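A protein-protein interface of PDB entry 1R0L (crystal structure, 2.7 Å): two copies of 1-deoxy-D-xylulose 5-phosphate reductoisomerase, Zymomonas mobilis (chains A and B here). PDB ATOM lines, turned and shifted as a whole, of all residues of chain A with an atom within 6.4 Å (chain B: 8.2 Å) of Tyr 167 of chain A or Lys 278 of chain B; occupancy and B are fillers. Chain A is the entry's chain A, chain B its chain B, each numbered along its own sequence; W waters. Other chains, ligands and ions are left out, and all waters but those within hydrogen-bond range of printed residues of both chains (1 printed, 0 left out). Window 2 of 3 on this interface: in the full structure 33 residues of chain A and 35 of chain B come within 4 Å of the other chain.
Pro 161 of chain A touches none of the printed residues of chain B.
Of the printed residues of chain B, Tyr 167 of chain A touches Lys 278 and Arg 279.
Of the printed residues of chain B, Arg 169 of chain A touches Glu 281.
Printed residues of chain B within 4 Å of Tyr 252 of chain A: Arg 279 (3.5 Å).
Printed residues of chain B within 4 Å of Leu 253 of chain A: Met 280 (3.7 Å) and Glu 281 (3.2 Å).
Printed residues of chain B within 4 Å of Asp 254 of chain A: Arg 279 (3.1 Å) and Met 280 (3.3 Å).
Arg 5 of chain B touches none of the printed residues of chain A.
Of the printed residues of chain A, Glu 281 of chain B touches Arg 169 (3.2 Å) and Leu 253 (3.2 Å).
The guanidinium group of Arg 169 of chain A sits at hydrogen-bond distance from the backbone carbonyl oxygen of Leu 253 of chain A.
The guanidinium group (NH1) of Arg 169 of chain A lies within salt-bridge range of the side-chain carboxylate (OE2) of Glu 251 of chain A.
The backbone carbonyl oxygen (O) of Tyr 167 of chain A sits at hydrogen-bond distance from the backbone NH (N) of Leu 253 of chain A (3.0 Å).
Printed residues of chain A that touch a printed residue of chain B: Tyr 167, Arg 169, Tyr 252, Leu 253 and Asp 254.
Hydrophobic or aromatic side chains of chain A that line the printed part of chain B: Tyr 167, Tyr 252 and Leu 253.
Along chain B the printed residues that touch a printed residue of chain A span positions 278 to 281.
Among the printed residues, Asp or Glu carboxylates within 4 Å of a Lys or Arg side-chain nitrogen of the other chain: Arg 169 of chain A with Glu 281 of chain B (3.2 Å) and Asp 254 of chain A with Arg 279 of chain B (3.1 Å).
Water W1 lies within hydrogen-bond range of OD2 of Asp 254 of chain A (2.7 Å), N of Met 280 of chain B (3.0 Å) and O of Gly 271 of chain B (3.2 Å).
No position is printed for both chains.
Of the 8 pairs that touch across the chains among the printed residues, none has its exchanged pair printed and touching as well.
Among the printed residues, pairs that only touch across the chains: Leu 253 of chain A with Glu 281 of chain B (3.2 Å), Tyr 167 of chain A with Lys 278 of chain B (3.4 Å), Tyr 252 of chain A with Arg 279 of chain B (3.5 Å), Tyr 167 of chain A with Arg 279 of chain B (3.6 Å) and Leu 253 of chain A with Met 280 of chain B (3.7 Å).
The guanidinium group (NH2) of Arg 169 of chain A is in salt-bridge range of the side-chain carboxylate (OE1) of Glu 281 of chain B (3.2 Å).
NH1 of Arg 279 of chain B is in salt-bridge range of OD2 of Asp 254 of chain A.
O of Met 280 of chain B lies close to N of Asp 254 of chain A (3.5 Å).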
ATOM      1  N   PRO A 161      14.191 -37.865   3.552  1.00  0.00           N
ATOM      2  CA  PRO A 161      14.290 -37.077   2.319  1.00  0.00           C
ATOM      3  C   PRO A 161      15.713 -37.168   1.759  1.00  0.00           C
ATOM      4  O   PRO A 161      16.551 -36.290   2.002  1.00  0.00           O
ATOM      5  CB  PRO A 161      13.927 -35.668   2.783  1.00  0.00           C
ATOM      6  CG  PRO A 161      14.520 -35.623   4.162  1.00  0.00           C
ATOM      7  CD  PRO A 161      14.175 -36.987   4.742  1.00  0.00           C
ATOM      8  N   ASN A 164      18.328 -34.372   0.502  1.00  0.00           N
ATOM      9  CA  ASN A 164      17.938 -33.169   1.232  1.00  0.00           C
ATOM     10  C   ASN A 164      17.968 -33.383   2.735  1.00  0.00           C
ATOM     11  O   ASN A 164      16.951 -33.212   3.398  1.00  0.00           O
ATOM     12  CB  ASN A 164      16.526 -32.745   0.835  1.00  0.00           C
ATOM     13  CG  ASN A 164      16.477 -32.098  -0.523  1.00  0.00           C
ATOM     14  OD1 ASN A 164      17.049 -31.028  -0.730  1.00  0.00           O
ATOM     15  ND2 ASN A 164      15.794 -32.740  -1.466  1.00  0.00           N
ATOM     16  N   ARG A 165      19.119 -33.755   3.280  1.00  0.00           N
ATOM     17  CA  ARG A 165      19.200 -33.979   4.718  1.00  0.00           C
ATOM     18  C   ARG A 165      18.849 -32.745   5.532  1.00  0.00           C
ATOM     19  O   ARG A 165      18.410 -32.860   6.671  1.00  0.00           O
ATOM     20  CB  ARG A 165      20.591 -34.459   5.129  1.00  0.00           C
ATOM     21  CG  ARG A 165      21.644 -34.254   4.105  1.00  0.00           C
ATOM     22  CD  ARG A 165      23.017 -34.382   4.731  1.00  0.00           C
ATOM     23  NE  ARG A 165      23.973 -34.789   3.713  1.00  0.00           N
ATOM     24  CZ  ARG A 165      23.946 -35.980   3.121  1.00  0.00           C
ATOM     25  NH1 ARG A 165      23.024 -36.867   3.465  1.00  0.00           N
ATOM     26  NH2 ARG A 165      24.814 -36.279   2.168  1.00  0.00           N
ATOM     27  N   ASP A 166      19.044 -31.563   4.958  1.00  0.00           N
ATOM     28  CA  ASP A 166      18.740 -30.344   5.692  1.00  0.00           C
ATOM     29  C   ASP A 166      17.246 -30.077   5.853  1.00  0.00           C
ATOM     30  O   ASP A 166      16.849 -29.065   6.426  1.00  0.00           O
ATOM     31  CB  ASP A 166      19.445 -29.147   5.057  1.00  0.00           C
ATOM     32  CG  ASP A 166      19.422 -29.191   3.565  1.00  0.00           C
ATOM     33  OD1 ASP A 166      18.307 -29.210   3.028  1.00  0.00           O
ATOM     34  OD2 ASP A 166      20.505 -29.208   2.931  1.00  0.00           O
ATOM     35  N   TYR A 167      16.425 -30.995   5.350  1.00  0.00           N
ATOM     36  CA  TYR A 167      14.973 -30.898   5.477  1.00  0.00           C
ATOM     37  C   TYR A 167      14.531 -31.575   6.778  1.00  0.00           C
ATOM     38  O   TYR A 167      13.414 -31.369   7.244  1.00  0.00           O
ATOM     39  CB  TYR A 167      14.277 -31.613   4.321  1.00  0.00           C
ATOM     40  CG  TYR A 167      14.170 -30.843   3.029  1.00  0.00           C
ATOM     41  CD1 TYR A 167      14.716 -29.573   2.900  1.00  0.00           C
ATOM     42  CD2 TYR A 167      13.529 -31.406   1.916  1.00  0.00           C
ATOM     43  CE1 TYR A 167      14.636 -28.873   1.691  1.00  0.00           C
ATOM     44  CE2 TYR A 167      13.443 -30.725   0.709  1.00  0.00           C
ATOM     45  CZ  TYR A 167      14.004 -29.454   0.598  1.00  0.00           C
ATOM     46  OH  TYR A 167      13.979 -28.782  -0.617  1.00  0.00           O
ATOM     47  N   VAL A 168      15.414 -32.383   7.353  1.00  0.00           N
ATOM     48  CA  VAL A 168      15.104 -33.113   8.574  1.00  0.00           C
ATOM     49  C   VAL A 168      15.338 -32.314   9.850  1.00  0.00           C
ATOM     50  O   VAL A 168      16.412 -31.769  10.070  1.00  0.00           O
ATOM     51  CB  VAL A 168      15.923 -34.443   8.636  1.00  0.00           C
ATOM     52  CG1 VAL A 168      15.598 -35.219   9.889  1.00  0.00           C
ATOM     53  CG2 VAL A 168      15.618 -35.298   7.414  1.00  0.00           C
ATOM     54  N   ARG A 169      14.316 -32.248  10.696  1.00  0.00           N
ATOM     55  CA  ARG A 169      14.431 -31.542  11.969  1.00  0.00           C
ATOM     56  C   ARG A 169      14.892 -32.516  13.043  1.00  0.00           C
ATOM     57  O   ARG A 169      15.590 -32.122  13.983  1.00  0.00           O
ATOM     58  CB  ARG A 169      13.095 -30.917  12.376  1.00  0.00           C
ATOM     59  CG  ARG A 169      13.088 -30.365  13.802  1.00  0.00           C
ATOM     60  CD  ARG A 169      11.831 -29.569  14.037  1.00  0.00           C
ATOM     61  NE  ARG A 169      11.734 -28.464  13.085  1.00  0.00           N
ATOM     62  CZ  ARG A 169      10.587 -27.942  12.663  1.00  0.00           C
ATOM     63  NH1 ARG A 169       9.429 -28.432  13.104  1.00  0.00           N
ATOM     64  NH2 ARG A 169      10.601 -26.920  11.816  1.00  0.00           N
ATOM     65  N   ARG A 170      14.495 -33.780  12.907  1.00  0.00           N
ATOM     66  CA  ARG A 170      14.917 -34.815  13.851  1.00  0.00           C
ATOM     67  C   ARG A 170      14.529 -36.210  13.375  1.00  0.00           C
ATOM     68  O   ARG A 170      13.615 -36.370  12.568  1.00  0.00           O
ATOM     69  CB  ARG A 170      14.315 -34.581  15.235  1.00  0.00           C
ATOM     70  CG  ARG A 170      12.821 -34.523  15.240  1.00  0.00           C
ATOM     71  CD  ARG A 170      12.283 -34.782  16.627  1.00  0.00           C
ATOM     72  NE  ARG A 170      10.869 -34.449  16.665  1.00  0.00           N
ATOM     73  CZ  ARG A 170      10.019 -34.842  17.602  1.00  0.00           C
ATOM     74  NH1 ARG A 170      10.434 -35.603  18.608  1.00  0.00           N
ATOM     75  NH2 ARG A 170       8.748 -34.466  17.520  1.00  0.00           N
ATOM     76  N   LYS A 235      20.321 -34.376  16.370  1.00  0.00           N
ATOM     77  CA  LYS A 235      19.030 -34.502  15.714  1.00  0.00           C
ATOM     78  C   LYS A 235      18.414 -35.878  15.927  1.00  0.00           C
ATOM     79  O   LYS A 235      17.251 -36.099  15.611  1.00  0.00           O
ATOM     80  CB  LYS A 235      19.154 -34.193  14.225  1.00  0.00           C
ATOM     81  CG  LYS A 235      19.565 -32.756  13.947  1.00  0.00           C
ATOM     82  CD  LYS A 235      19.359 -32.375  12.502  1.00  0.00           C
ATOM     83  CE  LYS A 235      19.381 -30.874  12.346  1.00  0.00           C
ATOM     84  NZ  LYS A 235      19.085 -30.478  10.953  1.00  0.00           N
ATOM     85  N   GLU A 251      11.033 -36.234  11.379  1.00  0.00           N
ATOM     86  CA  GLU A 251      10.281 -34.979  11.355  1.00  0.00           C
ATOM     87  C   GLU A 251      10.888 -33.972  10.398  1.00  0.00           C
ATOM     88  O   GLU A 251      12.085 -33.708  10.432  1.00  0.00           O
ATOM     89  CB  GLU A 251      10.213 -34.328  12.731  1.00  0.00           C
ATOM     90  CG  GLU A 251       9.300 -33.103  12.726  1.00  0.00           C
ATOM     91  CD  GLU A 251       9.216 -32.387  14.070  1.00  0.00           C
ATOM     92  OE1 GLU A 251       9.374 -33.048  15.124  1.00  0.00           O
ATOM     93  OE2 GLU A 251       8.964 -31.157  14.063  1.00  0.00           O
ATOM     94  N   TYR A 252      10.047 -33.404   9.549  1.00  0.00           N
ATOM     95  CA  TYR A 252      10.477 -32.410   8.576  1.00  0.00           C
ATOM     96  C   TYR A 252      10.365 -30.979   9.119  1.00  0.00           C
ATOM     97  O   TYR A 252       9.742 -30.725  10.159  1.00  0.00           O
ATOM     98  CB  TYR A 252       9.655 -32.545   7.295  1.00  0.00           C
ATOM     99  CG  TYR A 252       9.997 -33.782   6.511  1.00  0.00           C
ATOM    100  CD1 TYR A 252       9.944 -35.048   7.100  1.00  0.00           C
ATOM    101  CD2 TYR A 252      10.416 -33.690   5.186  1.00  0.00           C
ATOM    102  CE1 TYR A 252      10.311 -36.191   6.385  1.00  0.00           C
ATOM    103  CE2 TYR A 252      10.780 -34.824   4.460  1.00  0.00           C
ATOM    104  CZ  TYR A 252      10.728 -36.066   5.064  1.00  0.00           C
ATOM    105  OH  TYR A 252      11.097 -37.178   4.347  1.00  0.00           O
ATOM    106  N   LEU A 253      10.968 -30.049   8.390  1.00  0.00           N
ATOM    107  CA  LEU A 253      10.999 -28.655   8.775  1.00  0.00           C
ATOM    108  C   LEU A 253       9.641 -28.005   8.922  1.00  0.00           C
ATOM    109  O   LEU A 253       9.507 -27.011   9.646  1.00  0.00           O
ATOM    110  CB  LEU A 253      11.831 -27.865   7.770  1.00  0.00           C
ATOM    111  CG  LEU A 253      13.292 -28.298   7.613  1.00  0.00           C
ATOM    112  CD1 LEU A 253      13.904 -27.450   6.514  1.00  0.00           C
ATOM    113  CD2 LEU A 253      14.074 -28.149   8.927  1.00  0.00           C
ATOM    114  N   ASP A 254       8.631 -28.534   8.238  1.00  0.00           N
ATOM    115  CA  ASP A 254       7.309 -27.931   8.363  1.00  0.00           C
ATOM    116  C   ASP A 254       6.474 -28.524   9.493  1.00  0.00           C
ATOM    117  O   ASP A 254       5.276 -28.265   9.577  1.00  0.00           O
ATOM    118  CB  ASP A 254       6.541 -28.008   7.040  1.00  0.00           C
ATOM    119  CG  ASP A 254       6.534 -29.399   6.438  1.00  0.00           C
ATOM    120  OD1 ASP A 254       6.404 -30.382   7.201  1.00  0.00           O
ATOM    121  OD2 ASP A 254       6.641 -29.512   5.194  1.00  0.00           O
ATOM    122  N   ARG B   5       8.057 -16.671  -7.039  1.00  0.00           N
ATOM    123  CA  ARG B   5       6.987 -17.496  -7.563  1.00  0.00           C
ATOM    124  C   ARG B   5       5.659 -16.754  -7.357  1.00  0.00           C
ATOM    125  O   ARG B   5       5.312 -16.393  -6.228  1.00  0.00           O
ATOM    126  CB  ARG B   5       6.981 -18.829  -6.835  1.00  0.00           C
ATOM    127  CG  ARG B   5       6.034 -19.851  -7.403  1.00  0.00           C
ATOM    128  CD  ARG B   5       6.128 -21.099  -6.572  1.00  0.00           C
ATOM    129  NE  ARG B   5       5.216 -22.134  -7.015  1.00  0.00           N
ATOM    130  CZ  ARG B   5       4.942 -23.214  -6.299  1.00  0.00           C
ATOM    131  NH1 ARG B   5       5.525 -23.370  -5.115  1.00  0.00           N
ATOM    132  NH2 ARG B   5       4.082 -24.124  -6.759  1.00  0.00           N
ATOM    133  N   ARG B  30      10.198 -14.615  -1.542  1.00  0.00           N
ATOM    134  CA  ARG B  30      10.097 -15.742  -2.472  1.00  0.00           C
ATOM    135  C   ARG B  30       8.836 -15.723  -3.312  1.00  0.00           C
ATOM    136  O   ARG B  30       8.736 -16.432  -4.307  1.00  0.00           O
ATOM    137  CB  ARG B  30      10.019 -17.057  -1.724  1.00  0.00           C
ATOM    138  CG  ARG B  30      11.267 -17.646  -1.240  1.00  0.00           C
ATOM    139  CD  ARG B  30      10.902 -18.987  -0.653  1.00  0.00           C
ATOM    140  NE  ARG B  30      12.068 -19.681  -0.121  1.00  0.00           N
ATOM    141  CZ  ARG B  30      12.035 -20.874   0.471  1.00  0.00           C
ATOM    142  NH1 ARG B  30      10.880 -21.528   0.620  1.00  0.00           N
ATOM    143  NH2 ARG B  30      13.169 -21.420   0.901  1.00  0.00           N
ATOM    144  N   TYR B  31       7.850 -14.954  -2.877  1.00  0.00           N
ATOM    145  CA  TYR B  31       6.591 -14.938  -3.584  1.00  0.00           C
ATOM    146  C   TYR B  31       6.113 -13.562  -3.993  1.00  0.00           C
ATOM    147  O   TYR B  31       6.328 -12.571  -3.297  1.00  0.00           O
ATOM    148  CB  TYR B  31       5.519 -15.615  -2.724  1.00  0.00           C
ATOM    149  CG  TYR B  31       5.892 -17.001  -2.261  1.00  0.00           C
ATOM    150  CD1 TYR B  31       6.328 -17.239  -0.950  1.00  0.00           C
ATOM    151  CD2 TYR B  31       5.819 -18.086  -3.138  1.00  0.00           C
ATOM    152  CE1 TYR B  31       6.683 -18.531  -0.524  1.00  0.00           C
ATOM    153  CE2 TYR B  31       6.168 -19.376  -2.732  1.00  0.00           C
ATOM    154  CZ  TYR B  31       6.602 -19.596  -1.427  1.00  0.00           C
ATOM    155  OH  TYR B  31       6.966 -20.876  -1.050  1.00  0.00           O
ATOM    156  N   GLY B 271       1.968 -25.521   4.328  1.00  0.00           N
ATOM    157  CA  GLY B 271       3.384 -25.319   4.063  1.00  0.00           C
ATOM    158  C   GLY B 271       3.848 -26.365   3.069  1.00  0.00           C
ATOM    159  O   GLY B 271       4.621 -26.088   2.140  1.00  0.00           O
ATOM    160  N   HIS B 272       3.381 -27.593   3.266  1.00  0.00           N
ATOM    161  CA  HIS B 272       3.718 -28.671   2.348  1.00  0.00           C
ATOM    162  C   HIS B 272       3.286 -28.258   0.926  1.00  0.00           C
ATOM    163  O   HIS B 272       4.124 -28.151   0.037  1.00  0.00           O
ATOM    164  CB  HIS B 272       3.005 -29.957   2.777  1.00  0.00           C
ATOM    165  CG  HIS B 272       2.954 -31.009   1.711  1.00  0.00           C
ATOM    166  ND1 HIS B 272       4.033 -31.802   1.394  1.00  0.00           N
ATOM    167  CD2 HIS B 272       1.955 -31.385   0.879  1.00  0.00           C
ATOM    168  CE1 HIS B 272       3.703 -32.624   0.414  1.00  0.00           C
ATOM    169  NE2 HIS B 272       2.448 -32.392   0.085  1.00  0.00           N
ATOM    170  N   THR B 273       1.993 -27.991   0.719  1.00  0.00           N
ATOM    171  CA  THR B 273       1.495 -27.613  -0.605  1.00  0.00           C
ATOM    172  C   THR B 273       2.124 -26.357  -1.184  1.00  0.00           C
ATOM    173  O   THR B 273       2.173 -26.204  -2.414  1.00  0.00           O
ATOM    174  CB  THR B 273      -0.045 -27.394  -0.638  1.00  0.00           C
ATOM    175  OG1 THR B 273      -0.378 -26.187   0.055  1.00  0.00           O
ATOM    176  CG2 THR B 273      -0.774 -28.560   0.001  1.00  0.00           C
ATOM    177  N   LEU B 274       2.592 -25.456  -0.313  1.00  0.00           N
ATOM    178  CA  LEU B 274       3.212 -24.213  -0.773  1.00  0.00           C
ATOM    179  C   LEU B 274       4.659 -24.406  -1.228  1.00  0.00           C
ATOM    180  O   LEU B 274       5.121 -23.746  -2.154  1.00  0.00           O
ATOM    181  CB  LEU B 274       3.164 -23.160   0.330  1.00  0.00           C
ATOM    182  CG  LEU B 274       3.808 -21.814  -0.001  1.00  0.00           C
ATOM    183  CD1 LEU B 274       3.246 -21.234  -1.285  1.00  0.00           C
ATOM    184  CD2 LEU B 274       3.549 -20.875   1.148  1.00  0.00           C
ATOM    185  N   ALA B 275       5.373 -25.317  -0.585  1.00  0.00           N
ATOM    186  CA  ALA B 275       6.763 -25.549  -0.948  1.00  0.00           C
ATOM    187  C   ALA B 275       6.974 -26.694  -1.931  1.00  0.00           C
ATOM    188  O   ALA B 275       8.026 -26.776  -2.563  1.00  0.00           O
ATOM    189  CB  ALA B 275       7.597 -25.796   0.309  1.00  0.00           C
ATOM    190  N   TRP B 276       5.990 -27.579  -2.054  1.00  0.00           N
ATOM    191  CA  TRP B 276       6.083 -28.726  -2.965  1.00  0.00           C
ATOM    192  C   TRP B 276       6.601 -28.319  -4.352  1.00  0.00           C
ATOM    193  O   TRP B 276       6.106 -27.356  -4.949  1.00  0.00           O
ATOM    194  CB  TRP B 276       4.704 -29.380  -3.126  1.00  0.00           C
ATOM    195  CG  TRP B 276       4.761 -30.715  -3.791  1.00  0.00           C
ATOM    196  CD1 TRP B 276       4.891 -31.934  -3.182  1.00  0.00           C
ATOM    197  CD2 TRP B 276       4.756 -30.969  -5.199  1.00  0.00           C
ATOM    198  NE1 TRP B 276       4.969 -32.932  -4.123  1.00  0.00           N
ATOM    199  CE2 TRP B 276       4.888 -32.366  -5.372  1.00  0.00           C
ATOM    200  CE3 TRP B 276       4.656 -30.154  -6.331  1.00  0.00           C
ATOM    201  CZ2 TRP B 276       4.923 -32.965  -6.639  1.00  0.00           C
ATOM    202  CZ3 TRP B 276       4.692 -30.750  -7.592  1.00  0.00           C
ATOM    203  CH2 TRP B 276       4.825 -32.143  -7.732  1.00  0.00           C
ATOM    204  N   PRO B 277       7.548 -29.093  -4.915  1.00  0.00           N
ATOM    205  CA  PRO B 277       8.168 -30.315  -4.365  1.00  0.00           C
ATOM    206  C   PRO B 277       9.226 -30.161  -3.276  1.00  0.00           C
ATOM    207  O   PRO B 277       9.800 -31.145  -2.819  1.00  0.00           O
ATOM    208  CB  PRO B 277       8.737 -31.000  -5.602  1.00  0.00           C
ATOM    209  CG  PRO B 277       9.142 -29.822  -6.464  1.00  0.00           C
ATOM    210  CD  PRO B 277       7.965 -28.874  -6.316  1.00  0.00           C
ATOM    211  N   LYS B 278       9.495 -28.936  -2.859  1.00  0.00           N
ATOM    212  CA  LYS B 278      10.482 -28.726  -1.815  1.00  0.00           C
ATOM    213  C   LYS B 278       9.743 -28.593  -0.500  1.00  0.00           C
ATOM    214  O   LYS B 278       8.511 -28.570  -0.481  1.00  0.00           O
ATOM    215  CB  LYS B 278      11.279 -27.456  -2.095  1.00  0.00           C
ATOM    216  CG  LYS B 278      11.937 -27.407  -3.472  1.00  0.00           C
ATOM    217  CD  LYS B 278      12.664 -26.069  -3.640  1.00  0.00           C
ATOM    218  CE  LYS B 278      13.244 -25.874  -5.040  1.00  0.00           C
ATOM    219  NZ  LYS B 278      13.946 -24.542  -5.200  1.00  0.00           N
ATOM    220  N   ARG B 279      10.492 -28.522   0.595  1.00  0.00           N
ATOM    221  CA  ARG B 279       9.909 -28.350   1.918  1.00  0.00           C
ATOM    222  C   ARG B 279      10.335 -26.976   2.426  1.00  0.00           C
ATOM    223  O   ARG B 279      11.334 -26.419   1.957  1.00  0.00           O
ATOM    224  CB  ARG B 279      10.404 -29.434   2.866  1.00  0.00           C
ATOM    225  CG  ARG B 279       9.918 -30.816   2.507  1.00  0.00           C
ATOM    226  CD  ARG B 279       8.529 -31.080   3.046  1.00  0.00           C
ATOM    227  NE  ARG B 279       8.131 -32.462   2.787  1.00  0.00           N
ATOM    228  CZ  ARG B 279       7.195 -33.122   3.466  1.00  0.00           C
ATOM    229  NH1 ARG B 279       6.543 -32.537   4.466  1.00  0.00           N
ATOM    230  NH2 ARG B 279       6.909 -34.373   3.142  1.00  0.00           N
ATOM    231  N   MET B 280       9.573 -26.426   3.368  1.00  0.00           N
ATOM    232  CA  MET B 280       9.880 -25.117   3.921  1.00  0.00           C
ATOM    233  C   MET B 280       9.594 -25.116   5.412  1.00  0.00           C
ATOM    234  O   MET B 280       8.859 -25.974   5.915  1.00  0.00           O
ATOM    235  CB  MET B 280       9.039 -24.032   3.237  1.00  0.00           C
ATOM    236  CG  MET B 280       7.556 -24.203   3.467  1.00  0.00           C
ATOM    237  SD  MET B 280       6.518 -22.984   2.648  1.00  0.00           S
ATOM    238  CE  MET B 280       6.433 -21.716   3.942  1.00  0.00           C
ATOM    239  N   GLU B 281      10.194 -24.151   6.104  1.00  0.00           N
ATOM    240  CA  GLU B 281      10.030 -23.978   7.538  1.00  0.00           C
ATOM    241  C   GLU B 281       8.660 -23.372   7.806  1.00  0.00           C
ATOM    242  O   GLU B 281       8.199 -22.515   7.049  1.00  0.00           O
ATOM    243  CB  GLU B 281      11.089 -23.008   8.073  1.00  0.00           C
ATOM    244  CG  GLU B 281      12.446 -23.600   8.378  1.00  0.00           C
ATOM    245  CD  GLU B 281      12.447 -24.380   9.673  1.00  0.00           C
ATOM    246  OE1 GLU B 281      11.525 -24.162  10.487  1.00  0.00           O
ATOM    247  OE2 GLU B 281      13.373 -25.197   9.886  1.00  0.00           O
HETATM  248  O   HOH W   1       7.031 -27.974   3.046  1.00  0.00           O
